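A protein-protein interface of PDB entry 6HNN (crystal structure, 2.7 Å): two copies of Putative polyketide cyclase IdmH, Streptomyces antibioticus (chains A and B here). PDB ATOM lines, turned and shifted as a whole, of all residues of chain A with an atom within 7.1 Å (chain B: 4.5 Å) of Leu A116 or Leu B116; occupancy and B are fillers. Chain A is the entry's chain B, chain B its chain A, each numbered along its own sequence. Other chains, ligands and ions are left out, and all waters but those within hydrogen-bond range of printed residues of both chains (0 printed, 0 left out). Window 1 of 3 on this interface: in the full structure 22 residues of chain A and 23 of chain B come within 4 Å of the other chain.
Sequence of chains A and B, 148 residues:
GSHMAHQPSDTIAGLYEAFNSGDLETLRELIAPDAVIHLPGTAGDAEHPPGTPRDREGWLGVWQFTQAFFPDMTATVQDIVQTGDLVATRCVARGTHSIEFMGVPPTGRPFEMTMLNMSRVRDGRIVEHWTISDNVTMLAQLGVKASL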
ATOM      1  N   TYR A  16     -31.775 -40.520  -2.240  1.00  0.00           N
ATOM      2  CA  TYR A  16     -30.541 -40.634  -3.027  1.00  0.00           C
ATOM      3  C   TYR A  16     -30.171 -42.093  -3.335  1.00  0.00           C
ATOM      4  O   TYR A  16     -29.654 -42.360  -4.409  1.00  0.00           O
ATOM      5  CB  TYR A  16     -29.389 -39.799  -2.412  1.00  0.00           C
ATOM      6  CG  TYR A  16     -29.669 -38.307  -2.499  1.00  0.00           C
ATOM      7  CD1 TYR A  16     -29.811 -37.660  -3.735  1.00  0.00           C
ATOM      8  CD2 TYR A  16     -29.849 -37.551  -1.345  1.00  0.00           C
ATOM      9  CE1 TYR A  16     -30.069 -36.301  -3.823  1.00  0.00           C
ATOM     10  CE2 TYR A  16     -30.119 -36.173  -1.412  1.00  0.00           C
ATOM     11  CZ  TYR A  16     -30.227 -35.557  -2.650  1.00  0.00           C
ATOM     12  OH  TYR A  16     -30.497 -34.220  -2.743  1.00  0.00           O
ATOM     13  N   HIS A  38     -37.205 -26.682  -6.479  1.00  0.00           N
ATOM     14  CA  HIS A  38     -36.399 -25.559  -6.917  1.00  0.00           C
ATOM     15  C   HIS A  38     -35.063 -26.117  -7.404  1.00  0.00           C
ATOM     16  O   HIS A  38     -34.169 -26.390  -6.622  1.00  0.00           O
ATOM     17  CB  HIS A  38     -36.198 -24.565  -5.771  1.00  0.00           C
ATOM     18  CG  HIS A  38     -37.465 -24.073  -5.161  1.00  0.00           C
ATOM     19  ND1 HIS A  38     -38.237 -23.089  -5.741  1.00  0.00           N
ATOM     20  CD2 HIS A  38     -38.097 -24.426  -4.013  1.00  0.00           C
ATOM     21  CE1 HIS A  38     -39.295 -22.859  -4.977  1.00  0.00           C
ATOM     22  NE2 HIS A  38     -39.230 -23.655  -3.918  1.00  0.00           N
ATOM     23  N   ALA A  88     -31.032 -30.834   5.492  1.00  0.00           N
ATOM     24  CA  ALA A  88     -30.052 -30.270   4.580  1.00  0.00           C
ATOM     25  C   ALA A  88     -28.966 -31.277   4.403  1.00  0.00           C
ATOM     26  O   ALA A  88     -28.584 -31.934   5.356  1.00  0.00           O
ATOM     27  CB  ALA A  88     -29.467 -28.984   5.134  1.00  0.00           C
ATOM     28  N   THR A  89     -28.494 -31.427   3.175  1.00  0.00           N
ATOM     29  CA  THR A  89     -27.459 -32.395   2.860  1.00  0.00           C
ATOM     30  C   THR A  89     -26.380 -31.762   2.025  1.00  0.00           C
ATOM     31  O   THR A  89     -26.613 -30.812   1.308  1.00  0.00           O
ATOM     32  CB  THR A  89     -28.008 -33.637   2.111  1.00  0.00           C
ATOM     33  OG1 THR A  89     -28.879 -33.222   1.064  1.00  0.00           O
ATOM     34  CG2 THR A  89     -28.779 -34.533   3.024  1.00  0.00           C
ATOM     35  N   ARG A  90     -25.185 -32.308   2.155  1.00  0.00           N
ATOM     36  CA  ARG A  90     -24.092 -32.086   1.241  1.00  0.00           C
ATOM     37  C   ARG A  90     -23.829 -33.424   0.601  1.00  0.00           C
ATOM     38  O   ARG A  90     -23.675 -34.393   1.315  1.00  0.00           O
ATOM     39  CB  ARG A  90     -22.878 -31.599   2.007  1.00  0.00           C
ATOM     40  CG  ARG A  90     -21.670 -31.315   1.133  1.00  0.00           C
ATOM     41  CD  ARG A  90     -20.609 -30.594   1.946  1.00  0.00           C
ATOM     42  NE  ARG A  90     -19.991 -31.452   2.965  1.00  0.00           N
ATOM     43  CZ  ARG A  90     -19.046 -32.356   2.707  1.00  0.00           C
ATOM     44  NH1 ARG A  90     -18.591 -32.561   1.451  1.00  0.00           N
ATOM     45  NH2 ARG A  90     -18.560 -33.076   3.708  1.00  0.00           N
ATOM     46  N   CYS A  91     -23.824 -33.485  -0.718  1.00  0.00           N
ATOM     47  CA  CYS A  91     -23.525 -34.721  -1.446  1.00  0.00           C
ATOM     48  C   CYS A  91     -22.342 -34.520  -2.352  1.00  0.00           C
ATOM     49  O   CYS A  91     -21.891 -33.415  -2.566  1.00  0.00           O
ATOM     50  CB  CYS A  91     -24.699 -35.194  -2.300  1.00  0.00           C
ATOM     51  SG  CYS A  91     -26.231 -35.392  -1.425  1.00  0.00           S
ATOM     52  N   THR A 114     -19.593 -31.194  -5.765  1.00  0.00           N
ATOM     53  CA  THR A 114     -20.456 -30.964  -4.624  1.00  0.00           C
ATOM     54  C   THR A 114     -21.868 -30.582  -5.026  1.00  0.00           C
ATOM     55  O   THR A 114     -22.058 -29.803  -5.935  1.00  0.00           O
ATOM     56  CB  THR A 114     -19.868 -29.875  -3.719  1.00  0.00           C
ATOM     57  OG1 THR A 114     -18.599 -30.338  -3.254  1.00  0.00           O
ATOM     58  CG2 THR A 114     -20.733 -29.605  -2.484  1.00  0.00           C
ATOM     59  N   MET A 115     -22.842 -31.153  -4.343  1.00  0.00           N
ATOM     60  CA  MET A 115     -24.235 -30.708  -4.367  1.00  0.00           C
ATOM     61  C   MET A 115     -24.580 -30.298  -2.958  1.00  0.00           C
ATOM     62  O   MET A 115     -24.242 -30.994  -2.025  1.00  0.00           O
ATOM     63  CB  MET A 115     -25.172 -31.861  -4.742  1.00  0.00           C
ATOM     64  CG  MET A 115     -24.895 -32.585  -6.052  1.00  0.00           C
ATOM     65  SD  MET A 115     -26.312 -33.390  -6.830  1.00  0.00           S
ATOM     66  CE  MET A 115     -27.389 -33.834  -5.462  1.00  0.00           C
ATOM     67  N   LEU A 116     -25.283 -29.196  -2.800  1.00  0.00           N
ATOM     68  CA  LEU A 116     -25.937 -28.851  -1.540  1.00  0.00           C
ATOM     69  C   LEU A 116     -27.434 -28.897  -1.767  1.00  0.00           C
ATOM     70  O   LEU A 116     -27.908 -28.479  -2.794  1.00  0.00           O
ATOM     71  CB  LEU A 116     -25.507 -27.459  -1.085  1.00  0.00           C
ATOM     72  CG  LEU A 116     -24.031 -27.290  -0.751  1.00  0.00           C
ATOM     73  CD1 LEU A 116     -23.803 -25.860  -0.256  1.00  0.00           C
ATOM     74  CD2 LEU A 116     -23.572 -28.225   0.334  1.00  0.00           C
ATOM     75  N   ASN A 117     -28.172 -29.423  -0.807  1.00  0.00           N
ATOM     76  CA  ASN A 117     -29.622 -29.570  -0.893  1.00  0.00           C
ATOM     77  C   ASN A 117     -30.266 -29.199   0.426  1.00  0.00           C
ATOM     78  O   ASN A 117     -29.667 -29.353   1.477  1.00  0.00           O
ATOM     79  CB  ASN A 117     -30.027 -31.007  -1.227  1.00  0.00           C
ATOM     80  CG  ASN A 117     -29.149 -31.634  -2.286  1.00  0.00           C
ATOM     81  OD1 ASN A 117     -29.297 -31.371  -3.484  1.00  0.00           O
ATOM     82  ND2 ASN A 117     -28.248 -32.490  -1.860  1.00  0.00           N
ATOM     83  N   MET A 118     -31.494 -28.717   0.350  1.00  0.00           N
ATOM     84  CA  MET A 118     -32.357 -28.555   1.499  1.00  0.00           C
ATOM     85  C   MET A 118     -33.734 -29.039   1.102  1.00  0.00           C
ATOM     86  O   MET A 118     -34.193 -28.748   0.013  1.00  0.00           O
ATOM     87  CB  MET A 118     -32.401 -27.110   1.967  1.00  0.00           C
ATOM     88  CG  MET A 118     -33.050 -26.981   3.320  1.00  0.00           C
ATOM     89  SD  MET A 118     -32.663 -25.544   4.275  1.00  0.00           S
ATOM     90  CE  MET A 118     -30.881 -25.371   4.263  1.00  0.00           C
ATOM     91  N   HIS A 129     -38.117 -28.780  -2.070  1.00  0.00           N
ATOM     92  CA  HIS A 129     -36.717 -29.167  -2.251  1.00  0.00           C
ATOM     93  C   HIS A 129     -35.959 -28.083  -2.996  1.00  0.00           C
ATOM     94  O   HIS A 129     -36.433 -27.598  -4.007  1.00  0.00           O
ATOM     95  CB  HIS A 129     -36.681 -30.467  -3.019  1.00  0.00           C
ATOM     96  CG  HIS A 129     -35.321 -31.069  -3.137  1.00  0.00           C
ATOM     97  ND1 HIS A 129     -34.719 -31.728  -2.093  1.00  0.00           N
ATOM     98  CD2 HIS A 129     -34.476 -31.174  -4.198  1.00  0.00           C
ATOM     99  CE1 HIS A 129     -33.555 -32.199  -2.493  1.00  0.00           C
ATOM    100  NE2 HIS A 129     -33.381 -31.883  -3.769  1.00  0.00           N
ATOM    101  N   TRP A 130     -34.810 -27.697  -2.461  1.00  0.00           N
ATOM    102  CA  TRP A 130     -33.859 -26.812  -3.115  1.00  0.00           C
ATOM    103  C   TRP A 130     -32.587 -27.605  -3.332  1.00  0.00           C
ATOM    104  O   TRP A 130     -32.184 -28.367  -2.471  1.00  0.00           O
ATOM    105  CB  TRP A 130     -33.544 -25.623  -2.230  1.00  0.00           C
ATOM    106  CG  TRP A 130     -34.698 -24.717  -1.957  1.00  0.00           C
ATOM    107  CD1 TRP A 130     -35.009 -23.558  -2.622  1.00  0.00           C
ATOM    108  CD2 TRP A 130     -35.676 -24.867  -0.934  1.00  0.00           C
ATOM    109  NE1 TRP A 130     -36.134 -22.991  -2.071  1.00  0.00           N
ATOM    110  CE2 TRP A 130     -36.560 -23.771  -1.032  1.00  0.00           C
ATOM    111  CE3 TRP A 130     -35.900 -25.832   0.059  1.00  0.00           C
ATOM    112  CZ2 TRP A 130     -37.652 -23.604  -0.176  1.00  0.00           C
ATOM    113  CZ3 TRP A 130     -36.982 -25.669   0.934  1.00  0.00           C
ATOM    114  CH2 TRP A 130     -37.849 -24.564   0.805  1.00  0.00           C
ATOM    115  N   THR A 131     -31.959 -27.427  -4.487  1.00  0.00           N
ATOM    116  CA  THR A 131     -30.676 -28.065  -4.785  1.00  0.00           C
ATOM    117  C   THR A 131     -29.827 -27.194  -5.707  1.00  0.00           C
ATOM    118  O   THR A 131     -30.363 -26.519  -6.563  1.00  0.00           O
ATOM    119  CB  THR A 131     -30.885 -29.496  -5.365  1.00  0.00           C
ATOM    120  OG1 THR A 131     -29.627 -30.065  -5.738  1.00  0.00           O
ATOM    121  CG2 THR A 131     -31.800 -29.515  -6.556  1.00  0.00           C
ATOM    122  N   ILE A 132     -28.515 -27.187  -5.487  1.00  0.00           N
ATOM    123  CA  ILE A 132     -27.558 -26.559  -6.401  1.00  0.00           C
ATOM    124  C   ILE A 132     -26.310 -27.406  -6.446  1.00  0.00           C
ATOM    125  O   ILE A 132     -25.894 -27.948  -5.458  1.00  0.00           O
ATOM    126  CB  ILE A 132     -27.134 -25.124  -5.958  1.00  0.00           C
ATOM    127  CG1 ILE A 132     -28.320 -24.338  -5.366  1.00  0.00           C
ATOM    128  CG2 ILE A 132     -26.516 -24.372  -7.148  1.00  0.00           C
ATOM    129  CD1 ILE A 132     -27.959 -22.901  -5.066  1.00  0.00           C
ATOM    130  N   SER A 133     -25.717 -27.539  -7.625  1.00  0.00           N
ATOM    131  CA  SER A 133     -24.500 -28.308  -7.833  1.00  0.00           C
ATOM    132  C   SER A 133     -23.395 -27.400  -8.269  1.00  0.00           C
ATOM    133  O   SER A 133     -23.634 -26.384  -8.866  1.00  0.00           O
ATOM    134  CB  SER A 133     -24.749 -29.324  -8.925  1.00  0.00           C
ATOM    135  OG  SER A 133     -25.795 -30.204  -8.536  1.00  0.00           O
ATOM    136  N   ASP A 134     -22.163 -27.768  -7.974  1.00  0.00           N
ATOM    137  CA  ASP A 134     -20.998 -27.013  -8.404  1.00  0.00           C
ATOM    138  C   ASP A 134     -20.682 -27.362  -9.866  1.00  0.00           C
ATOM    139  O   ASP A 134     -19.741 -28.077 -10.189  1.00  0.00           O
ATOM    140  CB  ASP A 134     -19.815 -27.313  -7.492  1.00  0.00           C
ATOM    141  CG  ASP A 134     -18.673 -26.362  -7.646  1.00  0.00           C
ATOM    142  OD1 ASP A 134     -18.753 -25.465  -8.523  1.00  0.00           O
ATOM    143  OD2 ASP A 134     -17.689 -26.513  -6.880  1.00  0.00           O
ATOM    144  N   THR B  89     -27.885 -23.400   6.034  1.00  0.00           N
ATOM    145  CA  THR B  89     -28.793 -22.292   5.773  1.00  0.00           C
ATOM    146  C   THR B  89     -29.200 -22.266   4.327  1.00  0.00           C
ATOM    147  O   THR B  89     -28.475 -22.735   3.447  1.00  0.00           O
ATOM    148  CB  THR B  89     -28.165 -20.928   6.125  1.00  0.00           C
ATOM    149  OG1 THR B  89     -26.828 -20.852   5.606  1.00  0.00           O
ATOM    150  CG2 THR B  89     -28.143 -20.736   7.643  1.00  0.00           C
ATOM    151  N   ARG B  90     -30.385 -21.730   4.102  1.00  0.00           N
ATOM    152  CA  ARG B  90     -30.835 -21.323   2.789  1.00  0.00           C
ATOM    153  C   ARG B  90     -30.994 -19.825   2.899  1.00  0.00           C
ATOM    154  O   ARG B  90     -31.660 -19.352   3.813  1.00  0.00           O
ATOM    155  CB  ARG B  90     -32.151 -21.983   2.458  1.00  0.00           C
ATOM    156  CG  ARG B  90     -32.684 -21.622   1.089  1.00  0.00           C
ATOM    157  CD  ARG B  90     -33.860 -22.507   0.709  1.00  0.00           C
ATOM    158  NE  ARG B  90     -35.045 -22.225   1.524  1.00  0.00           N
ATOM    159  CZ  ARG B  90     -35.876 -21.200   1.348  1.00  0.00           C
ATOM    160  NH1 ARG B  90     -35.671 -20.318   0.389  1.00  0.00           N
ATOM    161  NH2 ARG B  90     -36.910 -21.070   2.160  1.00  0.00           N
ATOM    162  N   THR B 114     -31.048 -17.939  -4.845  1.00  0.00           N
ATOM    163  CA  THR B 114     -30.840 -18.832  -3.715  1.00  0.00           C
ATOM    164  C   THR B 114     -29.356 -19.081  -3.467  1.00  0.00           C
ATOM    165  O   THR B 114     -28.589 -19.276  -4.406  1.00  0.00           O
ATOM    166  CB  THR B 114     -31.525 -20.174  -3.961  1.00  0.00           C
ATOM    167  OG1 THR B 114     -32.921 -19.933  -4.173  1.00  0.00           O
ATOM    168  CG2 THR B 114     -31.349 -21.128  -2.765  1.00  0.00           C
ATOM    169  N   MET B 115     -28.979 -19.048  -2.193  1.00  0.00           N
ATOM    170  CA  MET B 115     -27.686 -19.531  -1.731  1.00  0.00           C
ATOM    171  C   MET B 115     -27.986 -20.666  -0.773  1.00  0.00           C
ATOM    172  O   MET B 115     -28.875 -20.535   0.061  1.00  0.00           O
ATOM    173  CB  MET B 115     -26.938 -18.477  -0.939  1.00  0.00           C
ATOM    174  CG  MET B 115     -26.689 -17.146  -1.619  1.00  0.00           C
ATOM    175  SD  MET B 115     -25.982 -15.917  -0.476  1.00  0.00           S
ATOM    176  CE  MET B 115     -24.824 -16.841   0.531  1.00  0.00           C
ATOM    177  N   LEU B 116     -27.266 -21.771  -0.907  1.00  0.00           N
ATOM    178  CA  LEU B 116     -27.285 -22.807   0.108  1.00  0.00           C
ATOM    179  C   LEU B 116     -25.918 -22.877   0.732  1.00  0.00           C
ATOM    180  O   LEU B 116     -24.912 -22.761   0.028  1.00  0.00           O
ATOM    181  CB  LEU B 116     -27.651 -24.163  -0.521  1.00  0.00           C
ATOM    182  CG  LEU B 116     -29.044 -24.262  -1.119  1.00  0.00           C
ATOM    183  CD1 LEU B 116     -29.267 -25.633  -1.706  1.00  0.00           C
ATOM    184  CD2 LEU B 116     -30.106 -24.016  -0.085  1.00  0.00           C
ATOM    185  N   ASN B 117     -25.874 -23.018   2.051  1.00  0.00           N
ATOM    186  CA  ASN B 117     -24.609 -23.048   2.793  1.00  0.00           C
ATOM    187  C   ASN B 117     -24.658 -24.120   3.857  1.00  0.00           C
ATOM    188  O   ASN B 117     -25.714 -24.436   4.375  1.00  0.00           O
ATOM    189  CB  ASN B 117     -24.326 -21.718   3.477  1.00  0.00           C
ATOM    190  CG  ASN B 117     -24.645 -20.527   2.607  1.00  0.00           C
ATOM    191  OD1 ASN B 117     -23.863 -20.172   1.727  1.00  0.00           O
ATOM    192  ND2 ASN B 117     -25.812 -19.881   2.862  1.00  0.00           N
ATOM    193  N   TRP B 130     -19.124 -24.595   3.385  1.00  0.00           N
ATOM    194  CA  TRP B 130     -19.448 -24.887   1.996  1.00  0.00           C
ATOM    195  C   TRP B 130     -20.543 -23.920   1.576  1.00  0.00           C
ATOM    196  O   TRP B 130     -21.454 -23.658   2.365  1.00  0.00           O
ATOM    197  CB  TRP B 130     -19.971 -26.303   1.867  1.00  0.00           C
ATOM    198  CG  TRP B 130     -18.986 -27.379   2.213  1.00  0.00           C
ATOM    199  CD1 TRP B 130     -18.196 -28.084   1.339  1.00  0.00           C
ATOM    200  CD2 TRP B 130     -18.704 -27.894   3.511  1.00  0.00           C
ATOM    201  NE1 TRP B 130     -17.439 -29.002   2.027  1.00  0.00           N
ATOM    202  CE2 TRP B 130     -17.732 -28.903   3.361  1.00  0.00           C
ATOM    203  CE3 TRP B 130     -19.172 -27.599   4.794  1.00  0.00           C
ATOM    204  CZ2 TRP B 130     -17.215 -29.620   4.459  1.00  0.00           C
ATOM    205  CZ3 TRP B 130     -18.655 -28.292   5.892  1.00  0.00           C
ATOM    206  CH2 TRP B 130     -17.696 -29.299   5.715  1.00  0.00           C
ATOM    207  N   THR B 131     -20.455 -23.385   0.360  1.00  0.00           N
ATOM    208  CA  THR B 131     -21.496 -22.491  -0.156  1.00  0.00           C
ATOM    209  C   THR B 131     -21.613 -22.593  -1.678  1.00  0.00           C
ATOM    210  O   THR B 131     -20.594 -22.779  -2.371  1.00  0.00           O
ATOM    211  CB  THR B 131     -21.255 -21.019   0.281  1.00  0.00           C
ATOM    212  OG1 THR B 131     -22.203 -20.142  -0.299  1.00  0.00           O
ATOM    213  CG2 THR B 131     -19.830 -20.540  -0.072  1.00  0.00           C
ATOM    214  N   ILE B 132     -22.838 -22.494  -2.197  1.00  0.00           N
ATOM    215  CA  ILE B 132     -23.083 -22.358  -3.635  1.00  0.00           C
ATOM    216  C   ILE B 132     -24.238 -21.385  -3.831  1.00  0.00           C
ATOM    217  O   ILE B 132     -25.196 -21.418  -3.061  1.00  0.00           O
ATOM    218  CB  ILE B 132     -23.452 -23.695  -4.320  1.00  0.00           C
ATOM    219  CG1 ILE B 132     -22.568 -24.828  -3.841  1.00  0.00           C
ATOM    220  CG2 ILE B 132     -23.281 -23.594  -5.828  1.00  0.00           C
ATOM    221  CD1 ILE B 132     -22.845 -26.164  -4.511  1.00  0.00           C
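Arg A90 touches Trp B130, and with the chains exchanged Trp A130 touches Arg B90.
Thr A114 touches Ile B132, and with the chains exchanged Ile A132 touches Thr B114.
Leu B116 touches its own counterpart, Leu A116.
Leu A116 touches Ile B132, and with the chains exchanged Ile A132 touches Leu B116.
Positions printed for both chains: 89, 90, 114, 115, 116, 117, 130, 131 and 132.
Of the 12 pairs that touch across the chains among the printed residues, 8 have their exchanged pair printed and touching as well.
Among the printed residues, merely in contact across the chains: Arg A90 with Trp B130 (3.4 Å), Thr A114 with Ile B132 (3.99 Å), Leu A116 with Leu B116 (3.3 Å), Leu A116 with Ile B132 (3.9 Å), Met A118 with Thr B89 (3.5 Å), Met A118 with Arg B90 (3.7 Å), Trp A130 with Arg B90 (3.3 Å), Ile A132 with Thr B114 (3.7 Å), Ile A132 with Leu B116 (3.996 Å), Ile A132 with Ile B132 (3.6 Å), Ser A133 with Ile B132 (3.99 Å) and Asp A134 with Ile B132 (3.9 Å).
Of the 17 printed residues of chain A, 8 touch a printed residue of chain B.
Printed residues of chain A that touch a printed residue of chain B: Arg A90, Thr A114, Leu A116, Met A118, Trp A130, Ile A132, Ser A133 and Asp A134.
Along chain B the printed residues that touch a printed residue of chain A span positions 89 to 132.
The backbone carbonyl oxygen (O) of Asn B117 sits at hydrogen-bond distance from the backbone NH (N) of Thr B89.
The backbone NH (N) of Trp A130 is in hydrogen-bond range of the backbone carbonyl oxygen (O) of Met A118 (2.8 Å).
The backbone NH (N) of Leu A116 lies within hydrogen-bond range of the backbone carbonyl oxygen (O) of Ile A132 (3.0 Å).
The backbone carbonyl oxygen of Thr A114 lies within hydrogen-bond range of the backbone NH of Asp A134, 2.9 Å away.
The side-chain sulfur (SD) of Met A115 sits close to the side-chain hydroxyl (OG) of Ser A133 (3.7 Å).
N of Leu B116 is in hydrogen-bond range of O of Ile B132, 3.0 Å away.
Ala A88 touches none of the printed residues of chain B.
Thr A89 touches none of the printed residues of chain B.
Of the printed residues of chain B, Arg A90 touches Trp B130.
Of the printed residues of chain B, Thr A114 touches Ile B132.
Printed residues of chain B within 4 Å of Met A118: Thr B89 (3.5 Å) and Arg B90 (3.7 Å).
Printed residues of chain B within 4 Å of Ser A133: Ile B132.
Printed residues of chain A within 4 Å of Leu B116: Leu A116 and Ile A132.
Printed residues of chain A within 4 Å of Trp B130: Arg A90 (3.4 Å).
The nearest residue of chain B that does not touch Leu A116 is Thr B131 (4.1 Å).
The nearest printed residue of chain A that does not touch Leu B116 is Asn A117 (4.04 Å).
The nearest printed residue of chain B that does not touch Arg A90 is Thr B131 (7.4 Å).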
